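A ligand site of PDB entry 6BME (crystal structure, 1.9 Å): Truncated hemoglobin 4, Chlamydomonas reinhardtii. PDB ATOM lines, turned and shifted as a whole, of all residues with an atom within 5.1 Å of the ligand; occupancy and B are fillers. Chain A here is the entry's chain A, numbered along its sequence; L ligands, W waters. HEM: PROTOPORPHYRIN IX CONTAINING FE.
The backbone carbonyl oxygen (O) of Ile 65 sits at hydrogen-bond distance from a ring nitrogen (ND1) of His 69. The backbone NH (N) of Leu 78 lies within hydrogen-bond range of the backbone carbonyl oxygen (O) of Leu 72, 3.0 Å away.
Water W3 lies within hydrogen-bond range of O2D of the ligand (2.4 Å) and NE2 of His 71 (2.9 Å).
FE of the ligand is bound by NE2 of His 69, 2.0 Å away. NZ of Lys 45 is bound to FE of the ligand (2.1 Å). An oxygen (O2A) of the ligand lies close to the backbone carbonyl oxygen of Thr 41.
Phe 33 touches the ligand (O to CMD, 3.2 Å). Phe 34 touches the ligand. Ala 44 touches the ligand. Arg 48 touches the ligand (CB to CMA, 3.7 Å). Phe 49 touches the ligand (CD2 to C2B, 3.4 Å). Tyr 60 touches the ligand (OH to CHB, 3.4 Å). His 71 touches the ligand (NE2 to O2D, 3.6 Å). Leu 72 touches the ligand (CD1 to CMD, 3.7 Å). Leu 78 touches the ligand. Phe 83 touches the ligand (CA to CMC, 3.6 Å). CG2 of Val 86 touches CMC of the ligand, 3.6 Å away. Leu 111 touches the ligand. Val 114 touches the ligand (CG2 to CBB, 3.6 Å). Phe 118 touches the ligand (CZ to CHC, 3.5 Å). Of the 23 residues printed, 17 come within 4 Å of the ligand. Along chain A the residues within 4 Å of the ligand span positions 33 to 118.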
ATOM      1  N   LEU A  30      -3.588   4.311 -23.077  1.00  0.00           N
ATOM      2  CA  LEU A  30      -4.362   4.255 -21.843  1.00  0.00           C
ATOM      3  C   LEU A  30      -5.869   4.298 -22.057  1.00  0.00           C
ATOM      4  O   LEU A  30      -6.612   3.657 -21.313  1.00  0.00           O
ATOM      5  CB  LEU A  30      -3.975   5.400 -20.924  1.00  0.00           C
ATOM      6  CG  LEU A  30      -2.497   5.452 -20.530  1.00  0.00           C
ATOM      7  CD1 LEU A  30      -2.183   6.742 -19.814  1.00  0.00           C
ATOM      8  CD2 LEU A  30      -2.159   4.223 -19.658  1.00  0.00           C
ATOM      9  N   PHE A  33      -8.426   1.263 -21.559  1.00  0.00           N
ATOM     10  CA  PHE A  33      -8.836   0.820 -20.221  1.00  0.00           C
ATOM     11  C   PHE A  33     -10.060   1.566 -19.720  1.00  0.00           C
ATOM     12  O   PHE A  33     -10.711   1.097 -18.783  1.00  0.00           O
ATOM     13  CB  PHE A  33      -7.693   0.990 -19.214  1.00  0.00           C
ATOM     14  CG  PHE A  33      -6.549   0.062 -19.448  1.00  0.00           C
ATOM     15  CD1 PHE A  33      -6.656  -1.286 -19.092  1.00  0.00           C
ATOM     16  CD2 PHE A  33      -5.369   0.510 -20.036  1.00  0.00           C
ATOM     17  CE1 PHE A  33      -5.602  -2.176 -19.321  1.00  0.00           C
ATOM     18  CE2 PHE A  33      -4.318  -0.362 -20.275  1.00  0.00           C
ATOM     19  CZ  PHE A  33      -4.433  -1.718 -19.911  1.00  0.00           C
ATOM     20  N   PHE A  34     -10.396   2.710 -20.307  1.00  0.00           N
ATOM     21  CA  PHE A  34     -11.552   3.478 -19.861  1.00  0.00           C
ATOM     22  C   PHE A  34     -12.791   3.259 -20.711  1.00  0.00           C
ATOM     23  O   PHE A  34     -13.861   3.813 -20.401  1.00  0.00           O
ATOM     24  CB  PHE A  34     -11.170   4.970 -19.816  1.00  0.00           C
ATOM     25  CG  PHE A  34     -10.029   5.253 -18.874  1.00  0.00           C
ATOM     26  CD1 PHE A  34     -10.239   5.258 -17.504  1.00  0.00           C
ATOM     27  CD2 PHE A  34      -8.757   5.463 -19.350  1.00  0.00           C
ATOM     28  CE1 PHE A  34      -9.193   5.496 -16.630  1.00  0.00           C
ATOM     29  CE2 PHE A  34      -7.707   5.712 -18.497  1.00  0.00           C
ATOM     30  CZ  PHE A  34      -7.926   5.718 -17.123  1.00  0.00           C
ATOM     31  N   VAL A  37     -16.439   2.744 -19.187  1.00  0.00           N
ATOM     32  CA  VAL A  37     -16.534   3.318 -17.843  1.00  0.00           C
ATOM     33  C   VAL A  37     -17.301   4.631 -17.916  1.00  0.00           C
ATOM     34  O   VAL A  37     -16.881   5.567 -18.603  1.00  0.00           O
ATOM     35  CB  VAL A  37     -15.163   3.535 -17.212  1.00  0.00           C
ATOM     36  CG1 VAL A  37     -15.346   3.909 -15.736  1.00  0.00           C
ATOM     37  CG2 VAL A  37     -14.304   2.281 -17.340  1.00  0.00           C
ATOM     38  N   THR A  41     -18.205   7.878 -12.755  1.00  0.00           N
ATOM     39  CA  THR A  41     -17.178   7.047 -12.138  1.00  0.00           C
ATOM     40  C   THR A  41     -15.771   7.571 -12.461  1.00  0.00           C
ATOM     41  O   THR A  41     -14.914   7.613 -11.575  1.00  0.00           O
ATOM     42  CB  THR A  41     -17.330   5.599 -12.609  1.00  0.00           C
ATOM     43  OG1 THR A  41     -18.636   5.115 -12.230  1.00  0.00           O
ATOM     44  CG2 THR A  41     -16.256   4.721 -12.022  1.00  0.00           C
ATOM     45  N   ALA A  44     -15.016  10.861 -10.671  1.00  0.00           N
ATOM     46  CA  ALA A  44     -14.820  10.558  -9.250  1.00  0.00           C
ATOM     47  C   ALA A  44     -13.472   9.899  -9.025  1.00  0.00           C
ATOM     48  O   ALA A  44     -12.777  10.204  -8.047  1.00  0.00           O
ATOM     49  CB  ALA A  44     -15.952   9.670  -8.722  1.00  0.00           C
ATOM     50  N   LYS A  45     -13.086   8.989  -9.928  1.00  0.00           N
ATOM     51  CA  LYS A  45     -11.763   8.360  -9.834  1.00  0.00           C
ATOM     52  C   LYS A  45     -10.651   9.405  -9.837  1.00  0.00           C
ATOM     53  O   LYS A  45      -9.730   9.353  -9.009  1.00  0.00           O
ATOM     54  CB  LYS A  45     -11.569   7.389 -11.000  1.00  0.00           C
ATOM     55  CG  LYS A  45     -10.091   7.107 -11.304  1.00  0.00           C
ATOM     56  CD  LYS A  45      -9.953   6.094 -12.433  1.00  0.00           C
ATOM     57  CE  LYS A  45      -8.520   6.043 -12.977  1.00  0.00           C
ATOM     58  NZ  LYS A  45      -7.499   5.732 -11.929  1.00  0.00           N
ATOM     59  N   ARG A  48     -10.447  11.340  -6.594  1.00  0.00           N
ATOM     60  CA  ARG A  48      -9.901  10.574  -5.478  1.00  0.00           C
ATOM     61  C   ARG A  48      -8.415  10.294  -5.675  1.00  0.00           C
ATOM     62  O   ARG A  48      -7.649  10.282  -4.703  1.00  0.00           O
ATOM     63  CB  ARG A  48     -10.690   9.269  -5.317  1.00  0.00           C
ATOM     64  CG  ARG A  48     -10.624   8.705  -3.908  1.00  0.00           C
ATOM     65  CD  ARG A  48     -11.560   7.542  -3.691  1.00  0.00           C
ATOM     66  NE  ARG A  48     -11.665   7.223  -2.264  1.00  0.00           N
ATOM     67  CZ  ARG A  48     -12.213   6.118  -1.780  1.00  0.00           C
ATOM     68  NH1 ARG A  48     -12.698   5.191  -2.596  1.00  0.00           N
ATOM     69  NH2 ARG A  48     -12.242   5.924  -0.473  1.00  0.00           N
ATOM     70  N   PHE A  49      -7.990  10.077  -6.928  1.00  0.00           N
ATOM     71  CA  PHE A  49      -6.567   9.920  -7.243  1.00  0.00           C
ATOM     72  C   PHE A  49      -5.786  11.148  -6.809  1.00  0.00           C
ATOM     73  O   PHE A  49      -4.763  11.051  -6.125  1.00  0.00           O
ATOM     74  CB  PHE A  49      -6.418   9.690  -8.764  1.00  0.00           C
ATOM     75  CG  PHE A  49      -5.020   9.354  -9.235  1.00  0.00           C
ATOM     76  CD1 PHE A  49      -3.988  10.286  -9.161  1.00  0.00           C
ATOM     77  CD2 PHE A  49      -4.767   8.144  -9.866  1.00  0.00           C
ATOM     78  CE1 PHE A  49      -2.699   9.983  -9.616  1.00  0.00           C
ATOM     79  CE2 PHE A  49      -3.490   7.829 -10.321  1.00  0.00           C
ATOM     80  CZ  PHE A  49      -2.454   8.749 -10.204  1.00  0.00           C
ATOM     81  N   TYR A  52      -5.724  11.372  -3.031  1.00  0.00           N
ATOM     82  CA  TYR A  52      -4.808  10.375  -2.489  1.00  0.00           C
ATOM     83  C   TYR A  52      -3.354  10.816  -2.636  1.00  0.00           C
ATOM     84  O   TYR A  52      -2.558  10.679  -1.691  1.00  0.00           O
ATOM     85  CB  TYR A  52      -5.026   9.024  -3.188  1.00  0.00           C
ATOM     86  CG  TYR A  52      -4.175   7.913  -2.613  1.00  0.00           C
ATOM     87  CD1 TYR A  52      -4.515   7.310  -1.412  1.00  0.00           C
ATOM     88  CD2 TYR A  52      -3.032   7.473  -3.271  1.00  0.00           C
ATOM     89  CE1 TYR A  52      -3.729   6.301  -0.868  1.00  0.00           C
ATOM     90  CE2 TYR A  52      -2.249   6.460  -2.736  1.00  0.00           C
ATOM     91  CZ  TYR A  52      -2.601   5.884  -1.545  1.00  0.00           C
ATOM     92  OH  TYR A  52      -1.832   4.876  -1.019  1.00  0.00           O
ATOM     93  N   TYR A  60      -8.952   5.086   2.028  1.00  0.00           N
ATOM     94  CA  TYR A  60      -8.417   4.554   0.786  1.00  0.00           C
ATOM     95  C   TYR A  60      -6.971   4.161   0.997  1.00  0.00           C
ATOM     96  O   TYR A  60      -6.128   5.023   1.272  1.00  0.00           O
ATOM     97  CB  TYR A  60      -8.559   5.598  -0.336  1.00  0.00           C
ATOM     98  CG  TYR A  60      -8.368   5.018  -1.707  1.00  0.00           C
ATOM     99  CD1 TYR A  60      -9.260   4.087  -2.205  1.00  0.00           C
ATOM    100  CD2 TYR A  60      -7.316   5.401  -2.498  1.00  0.00           C
ATOM    101  CE1 TYR A  60      -9.113   3.561  -3.451  1.00  0.00           C
ATOM    102  CE2 TYR A  60      -7.155   4.908  -3.746  1.00  0.00           C
ATOM    103  CZ  TYR A  60      -8.048   3.979  -4.219  1.00  0.00           C
ATOM    104  OH  TYR A  60      -7.867   3.468  -5.464  1.00  0.00           O
ATOM    105  N   ILE A  65      -6.683   0.005  -3.516  1.00  0.00           N
ATOM    106  CA  ILE A  65      -6.158   0.186  -4.874  1.00  0.00           C
ATOM    107  C   ILE A  65      -6.082  -1.159  -5.595  1.00  0.00           C
ATOM    108  O   ILE A  65      -6.454  -1.265  -6.771  1.00  0.00           O
ATOM    109  CB  ILE A  65      -4.788   0.881  -4.835  1.00  0.00           C
ATOM    110  CG1 ILE A  65      -4.938   2.293  -4.271  1.00  0.00           C
ATOM    111  CG2 ILE A  65      -4.179   0.908  -6.239  1.00  0.00           C
ATOM    112  CD1 ILE A  65      -3.642   2.946  -3.876  1.00  0.00           C
ATOM    113  N   GLY A  68      -9.590  -2.457  -6.479  1.00  0.00           N
ATOM    114  CA  GLY A  68     -10.197  -1.687  -7.558  1.00  0.00           C
ATOM    115  C   GLY A  68      -9.596  -1.932  -8.935  1.00  0.00           C
ATOM    116  O   GLY A  68     -10.271  -1.656  -9.941  1.00  0.00           O
ATOM    117  N   HIS A  69      -8.355  -2.422  -9.011  1.00  0.00           N
ATOM    118  CA  HIS A  69      -7.659  -2.564 -10.279  1.00  0.00           C
ATOM    119  C   HIS A  69      -7.270  -3.987 -10.633  1.00  0.00           C
ATOM    120  O   HIS A  69      -6.770  -4.201 -11.747  1.00  0.00           O
ATOM    121  CB  HIS A  69      -6.386  -1.689 -10.290  1.00  0.00           C
ATOM    122  CG  HIS A  69      -6.682  -0.224 -10.127  1.00  0.00           C
ATOM    123  ND1 HIS A  69      -6.907   0.353  -8.901  1.00  0.00           N
ATOM    124  CD2 HIS A  69      -6.836   0.763 -11.037  1.00  0.00           C
ATOM    125  CE1 HIS A  69      -7.175   1.633  -9.064  1.00  0.00           C
ATOM    126  NE2 HIS A  69      -7.138   1.908 -10.348  1.00  0.00           N
ATOM    127  N   HIS A  71      -8.825  -6.626 -11.545  1.00  0.00           N
ATOM    128  CA  HIS A  71      -9.411  -7.185 -12.757  1.00  0.00           C
ATOM    129  C   HIS A  71      -8.726  -6.660 -14.017  1.00  0.00           C
ATOM    130  O   HIS A  71      -8.646  -7.381 -15.019  1.00  0.00           O
ATOM    131  CB  HIS A  71     -10.920  -6.896 -12.792  1.00  0.00           C
ATOM    132  CG  HIS A  71     -11.274  -5.464 -13.056  1.00  0.00           C
ATOM    133  ND1 HIS A  71     -11.109  -4.474 -12.109  1.00  0.00           N
ATOM    134  CD2 HIS A  71     -11.796  -4.864 -14.147  1.00  0.00           C
ATOM    135  CE1 HIS A  71     -11.513  -3.319 -12.623  1.00  0.00           C
ATOM    136  NE2 HIS A  71     -11.938  -3.528 -13.852  1.00  0.00           N
ATOM    137  N   LEU A  72      -8.207  -5.419 -13.995  1.00  0.00           N
ATOM    138  CA  LEU A  72      -7.508  -4.889 -15.164  1.00  0.00           C
ATOM    139  C   LEU A  72      -6.158  -5.566 -15.352  1.00  0.00           C
ATOM    140  O   LEU A  72      -5.738  -5.826 -16.491  1.00  0.00           O
ATOM    141  CB  LEU A  72      -7.304  -3.377 -15.027  1.00  0.00           C
ATOM    142  CG  LEU A  72      -8.585  -2.573 -14.807  1.00  0.00           C
ATOM    143  CD1 LEU A  72      -8.284  -1.140 -14.393  1.00  0.00           C
ATOM    144  CD2 LEU A  72      -9.448  -2.594 -16.052  1.00  0.00           C
ATOM    145  N   LEU A  78      -3.133  -4.861 -17.692  1.00  0.00           N
ATOM    146  CA  LEU A  78      -2.651  -3.615 -17.087  1.00  0.00           C
ATOM    147  C   LEU A  78      -1.284  -3.843 -16.453  1.00  0.00           C
ATOM    148  O   LEU A  78      -1.086  -4.828 -15.738  1.00  0.00           O
ATOM    149  CB  LEU A  78      -3.651  -3.121 -16.040  1.00  0.00           C
ATOM    150  CG  LEU A  78      -3.310  -1.747 -15.447  1.00  0.00           C
ATOM    151  CD1 LEU A  78      -3.379  -0.750 -16.563  1.00  0.00           C
ATOM    152  CD2 LEU A  78      -4.271  -1.353 -14.297  1.00  0.00           C
ATOM    153  N   HIS A  82       1.819   1.087 -18.061  1.00  0.00           N
ATOM    154  CA  HIS A  82       0.599   1.878 -17.961  1.00  0.00           C
ATOM    155  C   HIS A  82       0.609   2.734 -16.705  1.00  0.00           C
ATOM    156  O   HIS A  82       0.293   3.934 -16.774  1.00  0.00           O
ATOM    157  CB  HIS A  82      -0.617   0.956 -17.984  1.00  0.00           C
ATOM    158  CG  HIS A  82      -0.708   0.129 -19.234  1.00  0.00           C
ATOM    159  ND1 HIS A  82      -0.907  -1.233 -19.201  1.00  0.00           N
ATOM    160  CD2 HIS A  82      -0.620   0.467 -20.540  1.00  0.00           C
ATOM    161  CE1 HIS A  82      -0.944  -1.695 -20.441  1.00  0.00           C
ATOM    162  NE2 HIS A  82      -0.761  -0.685 -21.265  1.00  0.00           N
ATOM    163  N   PHE A  83       1.004   2.162 -15.562  1.00  0.00           N
ATOM    164  CA  PHE A  83       1.079   2.932 -14.309  1.00  0.00           C
ATOM    165  C   PHE A  83       2.012   4.122 -14.455  1.00  0.00           C
ATOM    166  O   PHE A  83       1.689   5.227 -14.005  1.00  0.00           O
ATOM    167  CB  PHE A  83       1.555   2.057 -13.148  1.00  0.00           C
ATOM    168  CG  PHE A  83       1.772   2.835 -11.864  1.00  0.00           C
ATOM    169  CD1 PHE A  83       2.989   3.480 -11.616  1.00  0.00           C
ATOM    170  CD2 PHE A  83       0.766   2.932 -10.916  1.00  0.00           C
ATOM    171  CE1 PHE A  83       3.177   4.212 -10.453  1.00  0.00           C
ATOM    172  CE2 PHE A  83       0.946   3.656  -9.745  1.00  0.00           C
ATOM    173  CZ  PHE A  83       2.149   4.306  -9.506  1.00  0.00           C
ATOM    174  N   VAL A  86       0.324   6.897 -16.545  1.00  0.00           N
ATOM    175  CA  VAL A  86      -0.679   7.612 -15.763  1.00  0.00           C
ATOM    176  C   VAL A  86      -0.011   8.528 -14.748  1.00  0.00           C
ATOM    177  O   VAL A  86      -0.405   9.687 -14.584  1.00  0.00           O
ATOM    178  CB  VAL A  86      -1.635   6.599 -15.078  1.00  0.00           C
ATOM    179  CG1 VAL A  86      -2.476   7.286 -13.979  1.00  0.00           C
ATOM    180  CG2 VAL A  86      -2.549   5.927 -16.103  1.00  0.00           C
ATOM    181  N   LEU A 111       2.981   8.214  -5.231  1.00  0.00           N
ATOM    182  CA  LEU A 111       2.795   7.359  -6.409  1.00  0.00           C
ATOM    183  C   LEU A 111       3.844   6.269  -6.481  1.00  0.00           C
ATOM    184  O   LEU A 111       3.536   5.102  -6.763  1.00  0.00           O
ATOM    185  CB  LEU A 111       2.827   8.217  -7.673  1.00  0.00           C
ATOM    186  CG  LEU A 111       1.679   9.222  -7.781  1.00  0.00           C
ATOM    187  CD1 LEU A 111       1.787  10.078  -9.041  1.00  0.00           C
ATOM    188  CD2 LEU A 111       0.330   8.502  -7.703  1.00  0.00           C
ATOM    189  N   VAL A 114       3.025   3.304  -4.285  1.00  0.00           N
ATOM    190  CA  VAL A 114       2.017   2.335  -4.684  1.00  0.00           C
ATOM    191  C   VAL A 114       2.307   1.669  -6.023  1.00  0.00           C
ATOM    192  O   VAL A 114       1.583   0.731  -6.417  1.00  0.00           O
ATOM    193  CB  VAL A 114       0.604   2.972  -4.706  1.00  0.00           C
ATOM    194  CG1 VAL A 114       0.173   3.294  -3.301  1.00  0.00           C
ATOM    195  CG2 VAL A 114       0.580   4.211  -5.574  1.00  0.00           C
ATOM    196  N   PHE A 118       1.068  -2.478  -8.983  1.00  0.00           N
ATOM    197  CA  PHE A 118       0.732  -2.616 -10.393  1.00  0.00           C
ATOM    198  C   PHE A 118       1.722  -3.503 -11.130  1.00  0.00           C
ATOM    199  O   PHE A 118       1.713  -3.534 -12.362  1.00  0.00           O
ATOM    200  CB  PHE A 118       0.617  -1.228 -11.034  1.00  0.00           C
ATOM    201  CG  PHE A 118      -0.601  -0.481 -10.574  1.00  0.00           C
ATOM    202  CD1 PHE A 118      -0.589   0.205  -9.380  1.00  0.00           C
ATOM    203  CD2 PHE A 118      -1.782  -0.546 -11.316  1.00  0.00           C
ATOM    204  CE1 PHE A 118      -1.730   0.878  -8.923  1.00  0.00           C
ATOM    205  CE2 PHE A 118      -2.930   0.118 -10.875  1.00  0.00           C
ATOM    206  CZ  PHE A 118      -2.900   0.835  -9.670  1.00  0.00           C
HETATM  207  CHA HEM L   1     -10.710   2.938 -10.786  1.00  0.00           C
HETATM  208  CHB HEM L   1      -7.400   5.406  -8.266  1.00  0.00           C
HETATM  209  CHC HEM L   1      -4.020   3.689 -11.276  1.00  0.00           C
HETATM  210  CHD HEM L   1      -7.525   2.790 -14.472  1.00  0.00           C
HETATM  211  C1A HEM L   1     -10.152   3.727  -9.796  1.00  0.00           C
HETATM  212  C2A HEM L   1     -10.825   4.358  -8.664  1.00  0.00           C
HETATM  213  C3A HEM L   1      -9.871   5.048  -7.990  1.00  0.00           C
HETATM  214  C4A HEM L   1      -8.607   4.876  -8.661  1.00  0.00           C
HETATM  215  CMA HEM L   1     -10.035   5.880  -6.705  1.00  0.00           C
HETATM  216  CAA HEM L   1     -12.327   4.255  -8.285  1.00  0.00           C
HETATM  217  CBA HEM L   1     -13.243   4.802  -9.381  1.00  0.00           C
HETATM  218  CGA HEM L   1     -14.688   4.910  -8.940  1.00  0.00           C
HETATM  219  O1A HEM L   1     -15.322   3.860  -8.612  1.00  0.00           O
HETATM  220  O2A HEM L   1     -15.213   6.063  -8.952  1.00  0.00           O
HETATM  221  C1B HEM L   1      -6.168   5.044  -8.798  1.00  0.00           C
HETATM  222  C2B HEM L   1      -4.877   5.209  -8.163  1.00  0.00           C
HETATM  223  C3B HEM L   1      -3.949   4.716  -9.005  1.00  0.00           C
HETATM  224  C4B HEM L   1      -4.633   4.253 -10.193  1.00  0.00           C
HETATM  225  CMB HEM L   1      -4.622   5.825  -6.763  1.00  0.00           C
HETATM  226  CAB HEM L   1      -2.418   4.649  -8.862  1.00  0.00           C
HETATM  227  CBB HEM L   1      -1.709   5.457  -8.074  1.00  0.00           C
HETATM  228  C1C HEM L   1      -4.660   3.376 -12.448  1.00  0.00           C
HETATM  229  C2C HEM L   1      -4.039   3.067 -13.696  1.00  0.00           C
HETATM  230  C3C HEM L   1      -4.987   2.846 -14.600  1.00  0.00           C
HETATM  231  C4C HEM L   1      -6.268   2.978 -13.935  1.00  0.00           C
HETATM  232  CMC HEM L   1      -2.506   3.046 -13.929  1.00  0.00           C
HETATM  233  CAC HEM L   1      -4.716   2.500 -16.081  1.00  0.00           C
HETATM  234  CBC HEM L   1      -5.527   2.949 -17.041  1.00  0.00           C
HETATM  235  C1D HEM L   1      -8.684   2.670 -13.726  1.00  0.00           C
HETATM  236  C2D HEM L   1      -9.969   2.213 -14.204  1.00  0.00           C
HETATM  237  C3D HEM L   1     -10.840   2.262 -13.200  1.00  0.00           C
HETATM  238  C4D HEM L   1     -10.140   2.750 -12.034  1.00  0.00           C
HETATM  239  CMD HEM L   1     -10.256   1.772 -15.655  1.00  0.00           C
HETATM  240  CAD HEM L   1     -12.356   1.901 -13.210  1.00  0.00           C
HETATM  241  CBD HEM L   1     -12.539   0.397 -13.125  1.00  0.00           C
HETATM  242  CGD HEM L   1     -14.031   0.123 -13.209  1.00  0.00           C
HETATM  243  O1D HEM L   1     -14.812   0.903 -12.601  1.00  0.00           O
HETATM  244  O2D HEM L   1     -14.416  -0.873 -13.856  1.00  0.00           O
HETATM  245  NA  HEM L   1      -8.831   4.084  -9.760  1.00  0.00           N
HETATM  246  NB  HEM L   1      -5.991   4.448 -10.029  1.00  0.00           N
HETATM  247  NC  HEM L   1      -6.024   3.306 -12.622  1.00  0.00           N
HETATM  248  ND  HEM L   1      -8.818   2.986 -12.386  1.00  0.00           N
HETATM  249 FE   HEM L   1      -7.413   3.717 -11.216  1.00  0.00          FE
HETATM  250  O   HOH W   1     -13.959   1.777 -10.376  1.00  0.00           O
HETATM  251  O   HOH W   2     -11.998   2.454  -5.607  1.00  0.00           O
HETATM  252  O   HOH W   3     -13.080  -1.666 -15.745  1.00  0.00           O
HETATM  253  O   HOH W   4     -17.795   6.967  -8.165  1.00  0.00           O
